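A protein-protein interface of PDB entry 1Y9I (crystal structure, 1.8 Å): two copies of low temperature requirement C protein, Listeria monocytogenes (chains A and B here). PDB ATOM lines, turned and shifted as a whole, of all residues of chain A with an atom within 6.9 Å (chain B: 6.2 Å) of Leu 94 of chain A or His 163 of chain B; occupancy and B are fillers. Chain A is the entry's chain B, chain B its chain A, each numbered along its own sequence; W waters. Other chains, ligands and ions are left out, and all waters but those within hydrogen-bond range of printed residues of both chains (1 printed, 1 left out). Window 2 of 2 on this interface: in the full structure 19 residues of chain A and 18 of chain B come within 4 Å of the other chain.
Among the printed residues, pairs that only touch across the chains: Gly 93 of chain A with Ile 112 of chain B, Leu 94 of chain A with Ile 112 of chain B, Leu 94 of chain A with Ala 159 of chain B, Leu 94 of chain A with His 160 of chain B, Leu 94 of chain A with His 163 of chain B and Gly 96 of chain A with Ile 112 of chain B.
ND1 of His 160 of chain B lies within hydrogen-bond range of O of Ser 156 of chain B (3.1 Å).
Water W1 bridges O of Leu 94 of chain A and NE2 of His 160 of chain B.
Of chain B, only Ile 112 (3.6 Å), Ala 159 (3.9 Å), His 160 (3.96 Å) and His 163 (3.5 Å) come within 4 Å of Leu 94 of chain A.
His 163 of chain B touches just one residue of chain A: Leu 94 (3.5 Å).
Of the printed residues of chain B, Gly 96 of chain A touches Ile 112 (3.9 Å).
Of the printed residues of chain A, Ala 159 of chain B touches Leu 94 (3.9 Å).
Val 97 of chain A touches none of the printed residues of chain B.
The nearest residue of chain B that does not touch Leu 94 of chain A is Asp 164 of chain B (4.8 Å).
The nearest residue of chain A that does not touch His 163 of chain B is Glu 92 of chain A (4.5 Å).
Printed residues of chain A that touch a printed residue of chain B: Gly 93, Leu 94 and Gly 96.
Along chain A the printed residues that touch a printed residue of chain B span positions 93 to 96.
Of the 8 printed residues of chain B, 4 touch a printed residue of chain A.
Hydrophobic or aromatic side chains of chain B within 4 Å of the printed part of chain A: Ile 112, Ala 159, His 160 and His 163.
Among the printed residues, 6 pairs touch across the chains.
No position is printed for both chains.
Of the 6 pairs that touch across the chains among the printed residues, none has its exchanged pair printed and touching as well.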
ATOM      1  N   ILE A  87       8.466 -26.199  -9.508  1.00  0.00           N
ATOM      2  CA  ILE A  87       7.744 -27.181  -8.711  1.00  0.00           C
ATOM      3  C   ILE A  87       8.276 -28.597  -8.880  1.00  0.00           C
ATOM      4  O   ILE A  87       8.561 -29.279  -7.893  1.00  0.00           O
ATOM      5  CB  ILE A  87       6.232 -27.164  -9.047  1.00  0.00           C
ATOM      6  CG1 ILE A  87       5.624 -25.830  -8.603  1.00  0.00           C
ATOM      7  CG2 ILE A  87       5.526 -28.325  -8.348  1.00  0.00           C
ATOM      8  CD1 ILE A  87       4.177 -25.624  -9.057  1.00  0.00           C
ATOM      9  N   ASP A  91      10.982 -30.827  -6.552  1.00  0.00           N
ATOM     10  CA  ASP A  91      10.245 -31.929  -5.934  1.00  0.00           C
ATOM     11  C   ASP A  91       9.419 -31.391  -4.755  1.00  0.00           C
ATOM     12  O   ASP A  91       9.466 -31.926  -3.636  1.00  0.00           O
ATOM     13  CB  ASP A  91      11.221 -33.007  -5.457  1.00  0.00           C
ATOM     14  CG  ASP A  91      10.520 -34.281  -5.037  1.00  0.00           C
ATOM     15  OD1 ASP A  91       9.285 -34.365  -5.213  1.00  0.00           O
ATOM     16  OD2 ASP A  91      11.207 -35.198  -4.542  1.00  0.00           O
ATOM     17  N   GLU A  92       8.664 -30.329  -5.023  1.00  0.00           N
ATOM     18  CA  GLU A  92       7.828 -29.675  -4.019  1.00  0.00           C
ATOM     19  C   GLU A  92       6.959 -30.642  -3.226  1.00  0.00           C
ATOM     20  O   GLU A  92       6.274 -31.501  -3.793  1.00  0.00           O
ATOM     21  CB  GLU A  92       6.937 -28.620  -4.681  1.00  0.00           C
ATOM     22  CG  GLU A  92       7.675 -27.355  -5.098  1.00  0.00           C
ATOM     23  CD  GLU A  92       8.177 -26.564  -3.905  1.00  0.00           C
ATOM     24  OE1 GLU A  92       7.365 -26.285  -2.998  1.00  0.00           O
ATOM     25  OE2 GLU A  92       9.379 -26.221  -3.874  1.00  0.00           O
ATOM     26  N   GLY A  93       6.984 -30.476  -1.908  1.00  0.00           N
ATOM     27  CA  GLY A  93       6.221 -31.339  -1.028  1.00  0.00           C
ATOM     28  C   GLY A  93       4.728 -31.377  -1.288  1.00  0.00           C
ATOM     29  O   GLY A  93       4.103 -32.429  -1.129  1.00  0.00           O
ATOM     30  N   LEU A  94       4.145 -30.251  -1.693  1.00  0.00           N
ATOM     31  CA  LEU A  94       2.706 -30.213  -1.934  1.00  0.00           C
ATOM     32  C   LEU A  94       2.270 -30.566  -3.357  1.00  0.00           C
ATOM     33  O   LEU A  94       1.087 -30.463  -3.688  1.00  0.00           O
ATOM     34  CB  LEU A  94       2.149 -28.847  -1.529  1.00  0.00           C
ATOM     35  CG  LEU A  94       2.394 -28.495  -0.056  1.00  0.00           C
ATOM     36  CD1 LEU A  94       1.829 -27.110   0.235  1.00  0.00           C
ATOM     37  CD2 LEU A  94       1.759 -29.551   0.855  1.00  0.00           C
ATOM     38  N   TYR A  95       3.219 -30.978  -4.193  1.00  0.00           N
ATOM     39  CA  TYR A  95       2.916 -31.377  -5.566  1.00  0.00           C
ATOM     40  C   TYR A  95       2.701 -32.886  -5.502  1.00  0.00           C
ATOM     41  O   TYR A  95       3.632 -33.633  -5.202  1.00  0.00           O
ATOM     42  CB  TYR A  95       4.098 -31.054  -6.490  1.00  0.00           C
ATOM     43  CG  TYR A  95       3.865 -31.438  -7.942  1.00  0.00           C
ATOM     44  CD1 TYR A  95       3.043 -30.662  -8.774  1.00  0.00           C
ATOM     45  CD2 TYR A  95       4.477 -32.572  -8.490  1.00  0.00           C
ATOM     46  CE1 TYR A  95       2.847 -31.009 -10.127  1.00  0.00           C
ATOM     47  CE2 TYR A  95       4.283 -32.932  -9.838  1.00  0.00           C
ATOM     48  CZ  TYR A  95       3.472 -32.145 -10.646  1.00  0.00           C
ATOM     49  OH  TYR A  95       3.297 -32.488 -11.969  1.00  0.00           O
ATOM     50  N   GLY A  96       1.480 -33.341  -5.775  1.00  0.00           N
ATOM     51  CA  GLY A  96       1.218 -34.768  -5.678  1.00  0.00           C
ATOM     52  C   GLY A  96       0.906 -35.518  -6.957  1.00  0.00           C
ATOM     53  O   GLY A  96       0.428 -36.652  -6.907  1.00  0.00           O
ATOM     54  N   VAL A  97       1.193 -34.910  -8.104  1.00  0.00           N
ATOM     55  CA  VAL A  97       0.906 -35.568  -9.367  1.00  0.00           C
ATOM     56  C   VAL A  97       1.791 -36.789  -9.560  1.00  0.00           C
ATOM     57  O   VAL A  97       1.361 -37.777 -10.160  1.00  0.00           O
ATOM     58  CB  VAL A  97       1.069 -34.589 -10.550  1.00  0.00           C
ATOM     59  CG1 VAL A  97       0.765 -35.291 -11.877  1.00  0.00           C
ATOM     60  CG2 VAL A  97       0.118 -33.419 -10.363  1.00  0.00           C
ATOM     61  N   GLU A  99       2.735 -38.780  -7.214  1.00  0.00           N
ATOM     62  CA  GLU A  99       2.152 -39.865  -6.421  1.00  0.00           C
ATOM     63  C   GLU A  99       0.895 -40.420  -7.110  1.00  0.00           C
ATOM     64  O   GLU A  99       0.586 -41.603  -6.997  1.00  0.00           O
ATOM     65  CB  GLU A  99       1.802 -39.383  -5.009  1.00  0.00           C
ATOM     66  CG  GLU A  99       3.024 -39.146  -4.106  1.00  0.00           C
ATOM     67  CD  GLU A  99       3.672 -37.785  -4.299  1.00  0.00           C
ATOM     68  OE1 GLU A  99       3.217 -37.017  -5.169  1.00  0.00           O
ATOM     69  OE2 GLU A  99       4.644 -37.478  -3.574  1.00  0.00           O
ATOM     70  N   ILE B 112      -0.900 -36.313  -1.673  1.00  0.00           N
ATOM     71  CA  ILE B 112       0.306 -36.174  -0.863  1.00  0.00           C
ATOM     72  C   ILE B 112       0.209 -36.944   0.455  1.00  0.00           C
ATOM     73  O   ILE B 112       1.180 -37.038   1.204  1.00  0.00           O
ATOM     74  CB  ILE B 112       0.649 -34.704  -0.560  1.00  0.00           C
ATOM     75  CG1 ILE B 112      -0.420 -34.070   0.320  1.00  0.00           C
ATOM     76  CG2 ILE B 112       0.812 -33.934  -1.863  1.00  0.00           C
ATOM     77  CD1 ILE B 112       0.044 -32.765   0.937  1.00  0.00           C
ATOM     78  N   SER B 156      -1.578 -34.467   6.031  1.00  0.00           N
ATOM     79  CA  SER B 156      -1.613 -33.757   4.754  1.00  0.00           C
ATOM     80  C   SER B 156      -2.194 -32.357   4.940  1.00  0.00           C
ATOM     81  O   SER B 156      -1.678 -31.376   4.392  1.00  0.00           O
ATOM     82  CB  SER B 156      -2.455 -34.544   3.748  1.00  0.00           C
ATOM     83  OG  SER B 156      -2.654 -33.789   2.571  1.00  0.00           O
ATOM     84  N   ALA B 159       0.460 -30.292   6.412  1.00  0.00           N
ATOM     85  CA  ALA B 159       1.465 -29.918   5.418  1.00  0.00           C
ATOM     86  C   ALA B 159       0.996 -28.705   4.620  1.00  0.00           C
ATOM     87  O   ALA B 159       1.771 -27.773   4.376  1.00  0.00           O
ATOM     88  CB  ALA B 159       1.743 -31.082   4.482  1.00  0.00           C
ATOM     89  N   HIS B 160      -0.272 -28.715   4.216  1.00  0.00           N
ATOM     90  CA  HIS B 160      -0.828 -27.599   3.455  1.00  0.00           C
ATOM     91  C   HIS B 160      -0.934 -26.339   4.305  1.00  0.00           C
ATOM     92  O   HIS B 160      -0.941 -25.228   3.777  1.00  0.00           O
ATOM     93  CB  HIS B 160      -2.218 -27.937   2.908  1.00  0.00           C
ATOM     94  CG  HIS B 160      -2.196 -28.723   1.633  1.00  0.00           C
ATOM     95  ND1 HIS B 160      -2.086 -30.097   1.606  1.00  0.00           N
ATOM     96  CD2 HIS B 160      -2.257 -28.325   0.340  1.00  0.00           C
ATOM     97  CE1 HIS B 160      -2.082 -30.511   0.351  1.00  0.00           C
ATOM     98  NE2 HIS B 160      -2.184 -29.456  -0.436  1.00  0.00           N
ATOM     99  N   SER B 161      -1.014 -26.515   5.619  1.00  0.00           N
ATOM    100  CA  SER B 161      -1.134 -25.386   6.534  1.00  0.00           C
ATOM    101  C   SER B 161       0.077 -24.456   6.530  1.00  0.00           C
ATOM    102  O   SER B 161       0.081 -23.443   7.225  1.00  0.00           O
ATOM    103  CB  SER B 161      -1.384 -25.887   7.962  1.00  0.00           C
ATOM    104  OG  SER B 161      -2.606 -26.606   8.050  1.00  0.00           O
ATOM    105  N   TYR B 162       1.099 -24.791   5.751  1.00  0.00           N
ATOM    106  CA  TYR B 162       2.300 -23.958   5.686  1.00  0.00           C
ATOM    107  C   TYR B 162       2.435 -23.210   4.356  1.00  0.00           C
ATOM    108  O   TYR B 162       3.382 -22.444   4.154  1.00  0.00           O
ATOM    109  CB  TYR B 162       3.547 -24.815   5.928  1.00  0.00           C
ATOM    110  CG  TYR B 162       3.645 -25.384   7.329  1.00  0.00           C
ATOM    111  CD1 TYR B 162       2.663 -26.238   7.830  1.00  0.00           C
ATOM    112  CD2 TYR B 162       4.727 -25.073   8.154  1.00  0.00           C
ATOM    113  CE1 TYR B 162       2.756 -26.775   9.118  1.00  0.00           C
ATOM    114  CE2 TYR B 162       4.831 -25.600   9.442  1.00  0.00           C
ATOM    115  CZ  TYR B 162       3.842 -26.451   9.918  1.00  0.00           C
ATOM    116  OH  TYR B 162       3.939 -26.977  11.189  1.00  0.00           O
ATOM    117  N   HIS B 163       1.487 -23.436   3.452  1.00  0.00           N
ATOM    118  CA  HIS B 163       1.488 -22.780   2.145  1.00  0.00           C
ATOM    119  C   HIS B 163       0.097 -22.266   1.805  1.00  0.00           C
ATOM    120  O   HIS B 163      -0.062 -21.254   1.117  1.00  0.00           O
ATOM    121  CB  HIS B 163       1.932 -23.753   1.051  1.00  0.00           C
ATOM    122  CG  HIS B 163       3.416 -23.888   0.921  1.00  0.00           C
ATOM    123  ND1 HIS B 163       4.189 -24.561   1.843  1.00  0.00           N
ATOM    124  CD2 HIS B 163       4.270 -23.433  -0.027  1.00  0.00           C
ATOM    125  CE1 HIS B 163       5.456 -24.516   1.468  1.00  0.00           C
ATOM    126  NE2 HIS B 163       5.531 -23.838   0.336  1.00  0.00           N
ATOM    127  N   ASP B 164      -0.908 -22.979   2.295  1.00  0.00           N
ATOM    128  CA  ASP B 164      -2.298 -22.626   2.051  1.00  0.00           C
ATOM    129  C   ASP B 164      -2.970 -22.298   3.382  1.00  0.00           C
ATOM    130  O   ASP B 164      -4.000 -22.930   3.705  1.00  0.00           O
ATOM    131  CB  ASP B 164      -3.003 -23.802   1.367  1.00  0.00           C
ATOM    132  CG  ASP B 164      -2.272 -24.271   0.114  1.00  0.00           C
ATOM    133  OD1 ASP B 164      -2.581 -25.379  -0.382  1.00  0.00           O
ATOM    134  OD2 ASP B 164      -1.393 -23.527  -0.377  1.00  0.00           O
HETATM  135  O   HOH W   1      -1.559 -30.830  -3.144  1.00  0.00           O
